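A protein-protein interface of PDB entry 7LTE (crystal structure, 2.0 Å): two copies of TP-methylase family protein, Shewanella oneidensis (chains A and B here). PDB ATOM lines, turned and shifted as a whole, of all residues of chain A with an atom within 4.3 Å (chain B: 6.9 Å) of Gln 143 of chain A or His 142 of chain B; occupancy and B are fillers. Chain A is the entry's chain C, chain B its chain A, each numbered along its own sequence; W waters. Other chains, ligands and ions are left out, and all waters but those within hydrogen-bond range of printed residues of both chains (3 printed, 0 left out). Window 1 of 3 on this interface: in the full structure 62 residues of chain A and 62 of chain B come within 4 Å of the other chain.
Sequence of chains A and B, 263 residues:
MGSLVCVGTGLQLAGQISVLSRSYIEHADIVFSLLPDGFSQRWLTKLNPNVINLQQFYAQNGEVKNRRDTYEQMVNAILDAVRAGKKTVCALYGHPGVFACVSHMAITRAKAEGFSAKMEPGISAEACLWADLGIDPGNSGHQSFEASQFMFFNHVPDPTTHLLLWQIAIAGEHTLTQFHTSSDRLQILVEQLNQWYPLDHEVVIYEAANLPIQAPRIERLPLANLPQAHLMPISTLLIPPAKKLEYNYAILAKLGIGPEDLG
The backbone NH (N) of Ser 144 of chain B lies within hydrogen-bond range of the backbone carbonyl oxygen (O) of His 142 of chain A (2.9 Å). The backbone carbonyl oxygen (O) of His 142 of chain B lies within hydrogen-bond range of the backbone NH (N) of Ser 144 of chain A (2.9 Å). The backbone NH of Val 156 of chain A lies within hydrogen-bond range of the side-chain carboxylate of Asp 158 of chain B, 3.2 Å away. The backbone NH of Val 156 of chain B lies within hydrogen-bond range of the side-chain carboxylate of Asp 158 of chain A, 3.3 Å away. The side-chain amide oxygen of Gln 143 of chain A lies close to the side-chain amide oxygen of Gln 143 of chain B, 2.2 Å away.
O of His 162 of chain B sits at hydrogen-bond distance from N of Gln 143 of chain B. N of Leu 164 of chain A lies within hydrogen-bond range of O of Gln 143 of chain A, at 2.8 Å. NE2 of Gln 143 of chain B lies close to N of Asp 158 of chain B (2.9 Å). O of Gly 141 of chain B is in hydrogen-bond range of N of His 162 of chain B (3.0 Å). OG1 of Thr 161 of chain A is in hydrogen-bond range of NE2 of Gln 143 of chain A, 3.3 Å away. OG1 of Thr 161 of chain A is in hydrogen-bond range of O of Asp 158 of chain A (2.7 Å).
CE1 of His 142 of chain A touches CE1 of His 142 of chain B (3.5 Å). His 142 of chain A touches Gln 143 of chain B (O to CA, 3.2 Å). Gln 143 of chain A touches His 142 of chain B. O of Ser 144 of chain A touches CA of Gly 141 of chain B (3.2 Å). CE1 of Phe 145 of chain A touches OD2 of Asp 158 of chain B (3.7 Å). Thr 161 of chain B touches Phe 145 of chain A (CG2 to CE1, 3.6 Å). OD2 of Asp 158 of chain A touches CE1 of Phe 145 of chain B, at 3.7 Å. Phe 145 of chain B touches Thr 161 of chain A (CE1 to CG2, 3.6 Å).
Gln 143 of chain A touches just these residues of chain B: His 142 (3.2 Å) and Gln 143 (2.2 Å). Printed residues of chain B within 4 Å of Ser 144 of chain A: Gly 141 (3.2 Å) and His 142 (2.9 Å). Of the printed residues of chain B, Asp 158 of chain A touches Phe 145 (3.7 Å) and Val 156 (3.3 Å). Of the printed residues of chain A, Gly 141 of chain B touches Ser 144 (3.2 Å). Of chain A, only His 142 (3.5 Å), Gln 143 (3.2 Å) and Ser 144 (2.9 Å) come within 4 Å of His 142 of chain B. Of the printed residues of chain A, Thr 161 of chain B touches Phe 145. The nearest printed residue of chain B that does not touch Gln 143 of chain A is Val 156 of chain B (4.7 Å). The nearest printed residue of chain A that does not touch His 142 of chain B is Phe 145 of chain A (5.0 Å). The nearest printed residue of chain A that does not touch Val 156 of chain B is Gln 143 of chain A (4.7 Å).
Of the 11 printed residues of chain A, 7 touch a printed residue of chain B. Among the printed residues, 13 pairs touch across the chains. Among the printed residues, no Asp or Glu carboxylate lies within 4 Å of a Lys or Arg side-chain nitrogen of the other chain.
Gln 143 of chain A touches its own counterpart, Gln 143 of chain B. Phe 145 of chain A touches Asp 158 of chain B, and with the chains exchanged Asp 158 of chain A touches Phe 145 of chain B. Phe 145 of chain A touches Thr 161 of chain B, and with the chains exchanged Thr 161 of chain A touches Phe 145 of chain B. Val 156 of chain A touches Asp 158 of chain B, and with the chains exchanged Asp 158 of chain A touches Val 156 of chain B.
Water W2 lies within hydrogen-bond range of the side-chain carboxylate of Glu 126 of chain B (2.7 Å), a ring nitrogen (ND1) of His 142 of chain A (2.8 Å) and the side-chain hydroxyl of Ser 144 of chain B (3.1 Å). Water W1 bridges O of Val 156 of chain A and O of Val 156 of chain B. Water W3 bridges ND1 of His 142 of chain B and OG of Ser 144 of chain A.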
ATOM      1  N   HIS A 142      26.306 -29.105  23.127  1.00  0.00           N
ATOM      2  CA  HIS A 142      26.778 -28.504  24.388  1.00  0.00           C
ATOM      3  C   HIS A 142      25.845 -28.938  25.533  1.00  0.00           C
ATOM      4  O   HIS A 142      24.640 -28.898  25.346  1.00  0.00           O
ATOM      5  CB  HIS A 142      26.879 -26.983  24.198  1.00  0.00           C
ATOM      6  CG  HIS A 142      26.817 -26.198  25.452  1.00  0.00           C
ATOM      7  ND1 HIS A 142      26.100 -25.024  25.534  1.00  0.00           N
ATOM      8  CD2 HIS A 142      27.369 -26.413  26.667  1.00  0.00           C
ATOM      9  CE1 HIS A 142      26.251 -24.519  26.729  1.00  0.00           C
ATOM     10  NE2 HIS A 142      27.014 -25.364  27.461  1.00  0.00           N
ATOM     11  N   GLN A 143      26.417 -29.286  26.682  1.00  0.00           N
ATOM     12  CA  GLN A 143      25.639 -29.491  27.925  1.00  0.00           C
ATOM     13  C   GLN A 143      26.336 -28.727  29.043  1.00  0.00           C
ATOM     14  O   GLN A 143      27.585 -28.781  29.112  1.00  0.00           O
ATOM     15  CB  GLN A 143      25.603 -30.985  28.301  1.00  0.00           C
ATOM     16  CG  GLN A 143      24.884 -31.867  27.334  1.00  0.00           C
ATOM     17  CD  GLN A 143      24.826 -33.308  27.837  1.00  0.00           C
ATOM     18  OE1 GLN A 143      23.766 -33.881  28.034  1.00  0.00           O
ATOM     19  NE2 GLN A 143      25.988 -33.881  28.035  1.00  0.00           N
ATOM     20  N   SER A 144      25.557 -28.103  29.896  1.00  0.00           N
ATOM     21  CA  SER A 144      25.993 -27.412  31.133  1.00  0.00           C
ATOM     22  C   SER A 144      25.216 -27.974  32.345  1.00  0.00           C
ATOM     23  O   SER A 144      24.037 -28.069  32.283  1.00  0.00           O
ATOM     24  CB  SER A 144      25.767 -25.948  31.038  1.00  0.00           C
ATOM     25  OG  SER A 144      26.788 -25.309  30.313  1.00  0.00           O
ATOM     26  N   PHE A 145      25.926 -28.263  33.413  1.00  0.00           N
ATOM     27  CA  PHE A 145      25.371 -28.592  34.728  1.00  0.00           C
ATOM     28  C   PHE A 145      26.200 -27.939  35.827  1.00  0.00           C
ATOM     29  O   PHE A 145      27.438 -27.833  35.667  1.00  0.00           O
ATOM     30  CB  PHE A 145      25.407 -30.102  34.988  1.00  0.00           C
ATOM     31  CG  PHE A 145      24.795 -30.946  33.899  1.00  0.00           C
ATOM     32  CD1 PHE A 145      23.421 -31.179  33.865  1.00  0.00           C
ATOM     33  CD2 PHE A 145      25.585 -31.500  32.933  1.00  0.00           C
ATOM     34  CE1 PHE A 145      22.873 -32.001  32.891  1.00  0.00           C
ATOM     35  CE2 PHE A 145      25.031 -32.314  31.947  1.00  0.00           C
ATOM     36  CZ  PHE A 145      23.684 -32.567  31.936  1.00  0.00           C
ATOM     37  N   VAL A 156      22.537 -37.374  33.045  1.00  0.00           N
ATOM     38  CA  VAL A 156      23.190 -38.250  32.049  1.00  0.00           C
ATOM     39  C   VAL A 156      23.787 -37.362  30.959  1.00  0.00           C
ATOM     40  O   VAL A 156      23.086 -36.757  30.152  1.00  0.00           O
ATOM     41  CB  VAL A 156      22.194 -39.284  31.493  1.00  0.00           C
ATOM     42  CG1 VAL A 156      22.853 -40.193  30.460  1.00  0.00           C
ATOM     43  CG2 VAL A 156      21.578 -40.118  32.623  1.00  0.00           C
ATOM     44  N   PRO A 157      25.127 -37.294  30.899  1.00  0.00           N
ATOM     45  CA  PRO A 157      25.814 -36.540  29.863  1.00  0.00           C
ATOM     46  C   PRO A 157      25.853 -37.294  28.532  1.00  0.00           C
ATOM     47  O   PRO A 157      25.870 -38.542  28.518  1.00  0.00           O
ATOM     48  CB  PRO A 157      27.226 -36.364  30.431  1.00  0.00           C
ATOM     49  CG  PRO A 157      27.437 -37.541  31.341  1.00  0.00           C
ATOM     50  CD  PRO A 157      26.061 -38.000  31.792  1.00  0.00           C
ATOM     51  N   ASP A 158      25.780 -36.556  27.438  1.00  0.00           N
ATOM     52  CA  ASP A 158      25.959 -37.063  26.069  1.00  0.00           C
ATOM     53  C   ASP A 158      27.435 -36.855  25.751  1.00  0.00           C
ATOM     54  O   ASP A 158      27.899 -35.728  25.546  1.00  0.00           O
ATOM     55  CB  ASP A 158      24.987 -36.383  25.096  1.00  0.00           C
ATOM     56  CG  ASP A 158      25.187 -36.770  23.645  1.00  0.00           C
ATOM     57  OD1 ASP A 158      26.257 -37.399  23.340  1.00  0.00           O
ATOM     58  OD2 ASP A 158      24.310 -36.398  22.810  1.00  0.00           O
ATOM     59  N   THR A 161      29.113 -34.435  23.142  1.00  0.00           N
ATOM     60  CA  THR A 161      29.024 -32.962  23.343  1.00  0.00           C
ATOM     61  C   THR A 161      30.270 -32.396  24.008  1.00  0.00           C
ATOM     62  O   THR A 161      31.096 -33.153  24.543  1.00  0.00           O
ATOM     63  CB  THR A 161      27.765 -32.568  24.136  1.00  0.00           C
ATOM     64  OG1 THR A 161      27.844 -33.046  25.473  1.00  0.00           O
ATOM     65  CG2 THR A 161      26.522 -33.091  23.472  1.00  0.00           C
ATOM     66  N   HIS A 162      30.398 -31.055  23.993  1.00  0.00           N
ATOM     67  CA  HIS A 162      31.242 -30.340  24.954  1.00  0.00           C
ATOM     68  C   HIS A 162      30.426 -30.218  26.239  1.00  0.00           C
ATOM     69  O   HIS A 162      29.298 -29.619  26.206  1.00  0.00           O
ATOM     70  CB  HIS A 162      31.693 -28.989  24.348  1.00  0.00           C
ATOM     71  CG  HIS A 162      32.802 -29.172  23.379  1.00  0.00           C
ATOM     72  ND1 HIS A 162      32.566 -29.411  22.038  1.00  0.00           N
ATOM     73  CD2 HIS A 162      34.141 -29.224  23.558  1.00  0.00           C
ATOM     74  CE1 HIS A 162      33.713 -29.544  21.403  1.00  0.00           C
ATOM     75  NE2 HIS A 162      34.726 -29.466  22.341  1.00  0.00           N
ATOM     76  N   LEU A 163      30.945 -30.743  27.334  1.00  0.00           N
ATOM     77  CA  LEU A 163      30.269 -30.704  28.649  1.00  0.00           C
ATOM     78  C   LEU A 163      30.970 -29.699  29.559  1.00  0.00           C
ATOM     79  O   LEU A 163      32.244 -29.821  29.744  1.00  0.00           O
ATOM     80  CB  LEU A 163      30.297 -32.125  29.219  1.00  0.00           C
ATOM     81  CG  LEU A 163      29.958 -32.287  30.683  1.00  0.00           C
ATOM     82  CD1 LEU A 163      28.519 -31.846  30.938  1.00  0.00           C
ATOM     83  CD2 LEU A 163      30.145 -33.752  31.103  1.00  0.00           C
ATOM     84  N   LEU A 164      30.186 -28.790  30.148  1.00  0.00           N
ATOM     85  CA  LEU A 164      30.696 -27.808  31.145  1.00  0.00           C
ATOM     86  C   LEU A 164      30.163 -28.204  32.530  1.00  0.00           C
ATOM     87  O   LEU A 164      28.937 -28.396  32.690  1.00  0.00           O
ATOM     88  CB  LEU A 164      30.225 -26.410  30.738  1.00  0.00           C
ATOM     89  CG  LEU A 164      30.785 -25.823  29.445  1.00  0.00           C
ATOM     90  CD1 LEU A 164      30.498 -24.348  29.349  1.00  0.00           C
ATOM     91  CD2 LEU A 164      32.285 -26.057  29.330  1.00  0.00           C
ATOM     92  N   GLU B 126      20.592 -17.517  22.668  1.00  0.00           N
ATOM     93  CA  GLU B 126      20.419 -18.341  23.914  1.00  0.00           C
ATOM     94  C   GLU B 126      20.492 -17.393  25.136  1.00  0.00           C
ATOM     95  O   GLU B 126      19.701 -17.548  26.102  1.00  0.00           O
ATOM     96  CB  GLU B 126      21.515 -19.408  23.988  1.00  0.00           C
ATOM     97  CG  GLU B 126      21.659 -20.148  25.319  1.00  0.00           C
ATOM     98  CD  GLU B 126      23.084 -20.513  25.769  1.00  0.00           C
ATOM     99  OE1 GLU B 126      23.799 -21.192  24.979  1.00  0.00           O
ATOM    100  OE2 GLU B 126      23.507 -20.111  26.910  1.00  0.00           O
ATOM    101  N   TRP B 130      17.280 -16.877  28.011  1.00  0.00           N
ATOM    102  CA  TRP B 130      17.307 -16.974  29.491  1.00  0.00           C
ATOM    103  C   TRP B 130      16.660 -15.754  30.103  1.00  0.00           C
ATOM    104  O   TRP B 130      15.887 -15.931  31.045  1.00  0.00           O
ATOM    105  CB  TRP B 130      18.691 -17.228  30.073  1.00  0.00           C
ATOM    106  CG  TRP B 130      19.474 -18.356  29.485  1.00  0.00           C
ATOM    107  CD1 TRP B 130      20.757 -18.286  28.994  1.00  0.00           C
ATOM    108  CD2 TRP B 130      19.007 -19.700  29.212  1.00  0.00           C
ATOM    109  NE1 TRP B 130      21.126 -19.511  28.475  1.00  0.00           N
ATOM    110  CE2 TRP B 130      20.085 -20.397  28.603  1.00  0.00           C
ATOM    111  CE3 TRP B 130      17.818 -20.395  29.449  1.00  0.00           C
ATOM    112  CZ2 TRP B 130      20.025 -21.759  28.283  1.00  0.00           C
ATOM    113  CZ3 TRP B 130      17.755 -21.748  29.143  1.00  0.00           C
ATOM    114  CH2 TRP B 130      18.839 -22.411  28.558  1.00  0.00           C
ATOM    115  N   ASP B 136      17.013 -19.901  34.217  1.00  0.00           N
ATOM    116  CA  ASP B 136      18.459 -20.099  34.472  1.00  0.00           C
ATOM    117  C   ASP B 136      18.912 -21.470  33.944  1.00  0.00           C
ATOM    118  O   ASP B 136      18.431 -22.486  34.376  1.00  0.00           O
ATOM    119  CB  ASP B 136      18.746 -19.987  35.980  1.00  0.00           C
ATOM    120  CG  ASP B 136      20.222 -20.032  36.316  1.00  0.00           C
ATOM    121  OD1 ASP B 136      21.022 -20.475  35.462  1.00  0.00           O
ATOM    122  OD2 ASP B 136      20.570 -19.616  37.424  1.00  0.00           O
ATOM    123  N   PRO B 137      19.878 -21.530  32.998  1.00  0.00           N
ATOM    124  CA  PRO B 137      20.405 -22.787  32.487  1.00  0.00           C
ATOM    125  C   PRO B 137      20.949 -23.693  33.596  1.00  0.00           C
ATOM    126  O   PRO B 137      20.920 -24.893  33.451  1.00  0.00           O
ATOM    127  CB  PRO B 137      21.553 -22.406  31.546  1.00  0.00           C
ATOM    128  CG  PRO B 137      21.858 -20.965  31.917  1.00  0.00           C
ATOM    129  CD  PRO B 137      20.555 -20.372  32.406  1.00  0.00           C
ATOM    130  N   GLY B 138      21.369 -23.109  34.714  1.00  0.00           N
ATOM    131  CA  GLY B 138      21.871 -23.900  35.854  1.00  0.00           C
ATOM    132  C   GLY B 138      20.764 -24.553  36.684  1.00  0.00           C
ATOM    133  O   GLY B 138      21.077 -25.463  37.489  1.00  0.00           O
ATOM    134  N   ASN B 139      19.519 -24.101  36.547  1.00  0.00           N
ATOM    135  CA  ASN B 139      18.447 -24.499  37.509  1.00  0.00           C
ATOM    136  C   ASN B 139      18.322 -26.016  37.477  1.00  0.00           C
ATOM    137  O   ASN B 139      18.341 -26.611  38.537  1.00  0.00           O
ATOM    138  CB  ASN B 139      17.106 -23.868  37.164  1.00  0.00           C
ATOM    139  CG  ASN B 139      16.073 -24.223  38.201  1.00  0.00           C
ATOM    140  OD1 ASN B 139      16.016 -23.599  39.238  1.00  0.00           O
ATOM    141  ND2 ASN B 139      15.242 -25.195  37.884  1.00  0.00           N
ATOM    142  N   SER B 140      18.267 -26.606  36.291  1.00  0.00           N
ATOM    143  CA  SER B 140      18.279 -28.106  36.145  1.00  0.00           C
ATOM    144  C   SER B 140      19.231 -28.501  35.017  1.00  0.00           C
ATOM    145  O   SER B 140      19.195 -29.639  34.606  1.00  0.00           O
ATOM    146  CB  SER B 140      16.904 -28.674  35.998  1.00  0.00           C
ATOM    147  OG  SER B 140      16.226 -28.165  34.907  1.00  0.00           O
ATOM    148  N   GLY B 141      20.081 -27.548  34.578  1.00  0.00           N
ATOM    149  CA  GLY B 141      21.061 -27.767  33.490  1.00  0.00           C
ATOM    150  C   GLY B 141      20.513 -27.458  32.112  1.00  0.00           C
ATOM    151  O   GLY B 141      19.335 -27.254  31.916  1.00  0.00           O
ATOM    152  N   HIS B 142      21.412 -27.466  31.125  1.00  0.00           N
ATOM    153  CA  HIS B 142      21.077 -27.035  29.754  1.00  0.00           C
ATOM    154  C   HIS B 142      21.747 -27.920  28.711  1.00  0.00           C
ATOM    155  O   HIS B 142      22.865 -28.318  28.916  1.00  0.00           O
ATOM    156  CB  HIS B 142      21.480 -25.558  29.678  1.00  0.00           C
ATOM    157  CG  HIS B 142      21.733 -25.068  28.306  1.00  0.00           C
ATOM    158  ND1 HIS B 142      22.806 -24.223  28.021  1.00  0.00           N
ATOM    159  CD2 HIS B 142      21.091 -25.290  27.135  1.00  0.00           C
ATOM    160  CE1 HIS B 142      22.806 -23.936  26.721  1.00  0.00           C
ATOM    161  NE2 HIS B 142      21.772 -24.555  26.156  1.00  0.00           N
ATOM    162  N   GLN B 143      21.052 -28.212  27.622  1.00  0.00           N
ATOM    163  CA  GLN B 143      21.629 -28.905  26.436  1.00  0.00           C
ATOM    164  C   GLN B 143      21.193 -28.184  25.171  1.00  0.00           C
ATOM    165  O   GLN B 143      19.997 -27.766  25.082  1.00  0.00           O
ATOM    166  CB  GLN B 143      21.102 -30.335  26.325  1.00  0.00           C
ATOM    167  CG  GLN B 143      21.484 -31.218  27.474  1.00  0.00           C
ATOM    168  CD  GLN B 143      20.970 -32.630  27.240  1.00  0.00           C
ATOM    169  OE1 GLN B 143      21.741 -33.587  27.157  1.00  0.00           O
ATOM    170  NE2 GLN B 143      19.682 -32.737  27.060  1.00  0.00           N
ATOM    171  N   SER B 144      22.116 -28.042  24.245  1.00  0.00           N
ATOM    172  CA  SER B 144      21.922 -27.375  22.934  1.00  0.00           C
ATOM    173  C   SER B 144      22.405 -28.326  21.846  1.00  0.00           C
ATOM    174  O   SER B 144      23.537 -28.835  21.982  1.00  0.00           O
ATOM    175  CB  SER B 144      22.666 -26.046  22.850  1.00  0.00           C
ATOM    176  OG  SER B 144      21.922 -24.989  23.424  1.00  0.00           O
ATOM    177  N   PHE B 145      21.571 -28.544  20.832  1.00  0.00           N
ATOM    178  CA  PHE B 145      21.942 -29.266  19.596  1.00  0.00           C
ATOM    179  C   PHE B 145      21.397 -28.508  18.391  1.00  0.00           C
ATOM    180  O   PHE B 145      20.310 -27.941  18.498  1.00  0.00           O
ATOM    181  CB  PHE B 145      21.393 -30.710  19.559  1.00  0.00           C
ATOM    182  CG  PHE B 145      21.760 -31.551  20.743  1.00  0.00           C
ATOM    183  CD1 PHE B 145      23.002 -32.174  20.827  1.00  0.00           C
ATOM    184  CD2 PHE B 145      20.849 -31.785  21.760  1.00  0.00           C
ATOM    185  CE1 PHE B 145      23.318 -33.006  21.892  1.00  0.00           C
ATOM    186  CE2 PHE B 145      21.177 -32.601  22.844  1.00  0.00           C
ATOM    187  CZ  PHE B 145      22.417 -33.190  22.910  1.00  0.00           C
ATOM    188  N   VAL B 156      21.547 -38.111  22.745  1.00  0.00           N
ATOM    189  CA  VAL B 156      20.570 -38.511  23.789  1.00  0.00           C
ATOM    190  C   VAL B 156      20.381 -37.322  24.714  1.00  0.00           C
ATOM    191  O   VAL B 156      21.301 -36.843  25.380  1.00  0.00           O
ATOM    192  CB  VAL B 156      21.009 -39.797  24.537  1.00  0.00           C
ATOM    193  CG1 VAL B 156      20.108 -40.074  25.726  1.00  0.00           C
ATOM    194  CG2 VAL B 156      21.012 -40.997  23.593  1.00  0.00           C
ATOM    195  N   PRO B 157      19.156 -36.780  24.792  1.00  0.00           N
ATOM    196  CA  PRO B 157      18.896 -35.673  25.704  1.00  0.00           C
ATOM    197  C   PRO B 157      18.728 -36.192  27.138  1.00  0.00           C
ATOM    198  O   PRO B 157      18.218 -37.298  27.342  1.00  0.00           O
ATOM    199  CB  PRO B 157      17.633 -35.044  25.101  1.00  0.00           C
ATOM    200  CG  PRO B 157      16.886 -36.216  24.480  1.00  0.00           C
ATOM    201  CD  PRO B 157      17.974 -37.168  24.002  1.00  0.00           C
ATOM    202  N   ASP B 158      19.207 -35.422  28.110  1.00  0.00           N
ATOM    203  CA  ASP B 158      18.786 -35.551  29.526  1.00  0.00           C
ATOM    204  C   ASP B 158      17.482 -34.785  29.721  1.00  0.00           C
ATOM    205  O   ASP B 158      17.431 -33.561  29.638  1.00  0.00           O
ATOM    206  CB  ASP B 158      19.906 -35.065  30.432  1.00  0.00           C
ATOM    207  CG  ASP B 158      19.584 -35.056  31.915  1.00  0.00           C
ATOM    208  OD1 ASP B 158      18.412 -35.160  32.288  1.00  0.00           O
ATOM    209  OD2 ASP B 158      20.538 -34.896  32.661  1.00  0.00           O
ATOM    210  N   THR B 161      16.839 -31.491  31.906  1.00  0.00           N
ATOM    211  CA  THR B 161      17.448 -30.215  31.460  1.00  0.00           C
ATOM    212  C   THR B 161      16.482 -29.363  30.640  1.00  0.00           C
ATOM    213  O   THR B 161      15.430 -29.863  30.188  1.00  0.00           O
ATOM    214  CB  THR B 161      18.733 -30.432  30.657  1.00  0.00           C
ATOM    215  OG1 THR B 161      18.362 -30.986  29.395  1.00  0.00           O
ATOM    216  CG2 THR B 161      19.711 -31.305  31.402  1.00  0.00           C
ATOM    217  N   HIS B 162      16.792 -28.066  30.498  1.00  0.00           N
ATOM    218  CA  HIS B 162      16.221 -27.243  29.405  1.00  0.00           C
ATOM    219  C   HIS B 162      16.974 -27.568  28.122  1.00  0.00           C
ATOM    220  O   HIS B 162      18.223 -27.305  28.084  1.00  0.00           O
ATOM    221  CB  HIS B 162      16.273 -25.743  29.767  1.00  0.00           C
ATOM    222  CG  HIS B 162      15.247 -25.343  30.769  1.00  0.00           C
ATOM    223  ND1 HIS B 162      13.974 -24.897  30.418  1.00  0.00           N
ATOM    224  CD2 HIS B 162      15.324 -25.280  32.103  1.00  0.00           C
ATOM    225  CE1 HIS B 162      13.299 -24.660  31.506  1.00  0.00           C
ATOM    226  NE2 HIS B 162      14.082 -24.908  32.553  1.00  0.00           N
ATOM    227  N   LEU B 163      16.285 -28.141  27.134  1.00  0.00           N
ATOM    228  CA  LEU B 163      16.888 -28.598  25.862  1.00  0.00           C
ATOM    229  C   LEU B 163      16.567 -27.542  24.770  1.00  0.00           C
ATOM    230  O   LEU B 163      15.382 -27.146  24.584  1.00  0.00           O
ATOM    231  CB  LEU B 163      16.347 -30.003  25.512  1.00  0.00           C
ATOM    232  CG  LEU B 163      16.529 -30.444  24.057  1.00  0.00           C
ATOM    233  CD1 LEU B 163      18.000 -30.540  23.704  1.00  0.00           C
ATOM    234  CD2 LEU B 163      15.834 -31.784  23.805  1.00  0.00           C
ATOM    235  N   LEU B 164      17.588 -27.100  24.067  1.00  0.00           N
ATOM    236  CA  LEU B 164      17.417 -26.178  22.913  1.00  0.00           C
ATOM    237  C   LEU B 164      17.754 -26.913  21.619  1.00  0.00           C
ATOM    238  O   LEU B 164      18.883 -27.441  21.487  1.00  0.00           O
ATOM    239  CB  LEU B 164      18.302 -24.938  23.094  1.00  0.00           C
ATOM    240  CG  LEU B 164      17.847 -23.933  24.157  1.00  0.00           C
ATOM    241  CD1 LEU B 164      18.744 -22.707  24.117  1.00  0.00           C
ATOM    242  CD2 LEU B 164      16.398 -23.531  23.891  1.00  0.00           C
ATOM    243  N   TRP B 166      18.423 -25.805  17.918  1.00  0.00           N
ATOM    244  CA  TRP B 166      18.710 -24.603  17.089  1.00  0.00           C
ATOM    245  C   TRP B 166      18.484 -24.908  15.611  1.00  0.00           C
ATOM    246  O   TRP B 166      18.529 -26.134  15.199  1.00  0.00           O
ATOM    247  CB  TRP B 166      20.155 -24.190  17.304  1.00  0.00           C
ATOM    248  CG  TRP B 166      20.522 -23.741  18.682  1.00  0.00           C
ATOM    249  CD1 TRP B 166      20.525 -24.489  19.827  1.00  0.00           C
ATOM    250  CD2 TRP B 166      21.054 -22.466  19.046  1.00  0.00           C
ATOM    251  NE1 TRP B 166      20.977 -23.748  20.889  1.00  0.00           N
ATOM    252  CE2 TRP B 166      21.323 -22.513  20.435  1.00  0.00           C
ATOM    253  CE3 TRP B 166      21.371 -21.300  18.336  1.00  0.00           C
ATOM    254  CZ2 TRP B 166      21.906 -21.434  21.123  1.00  0.00           C
ATOM    255  CZ3 TRP B 166      21.920 -20.217  19.026  1.00  0.00           C
ATOM    256  CH2 TRP B 166      22.184 -20.299  20.399  1.00  0.00           C
HETATM  257  O   HOH W   1      22.155 -37.880  27.845  1.00  0.00           O
HETATM  258  O   HOH W   2      24.545 -23.464  23.832  1.00  0.00           O
HETATM  259  O   HOH W   3      24.788 -23.137  29.726  1.00  0.00           O
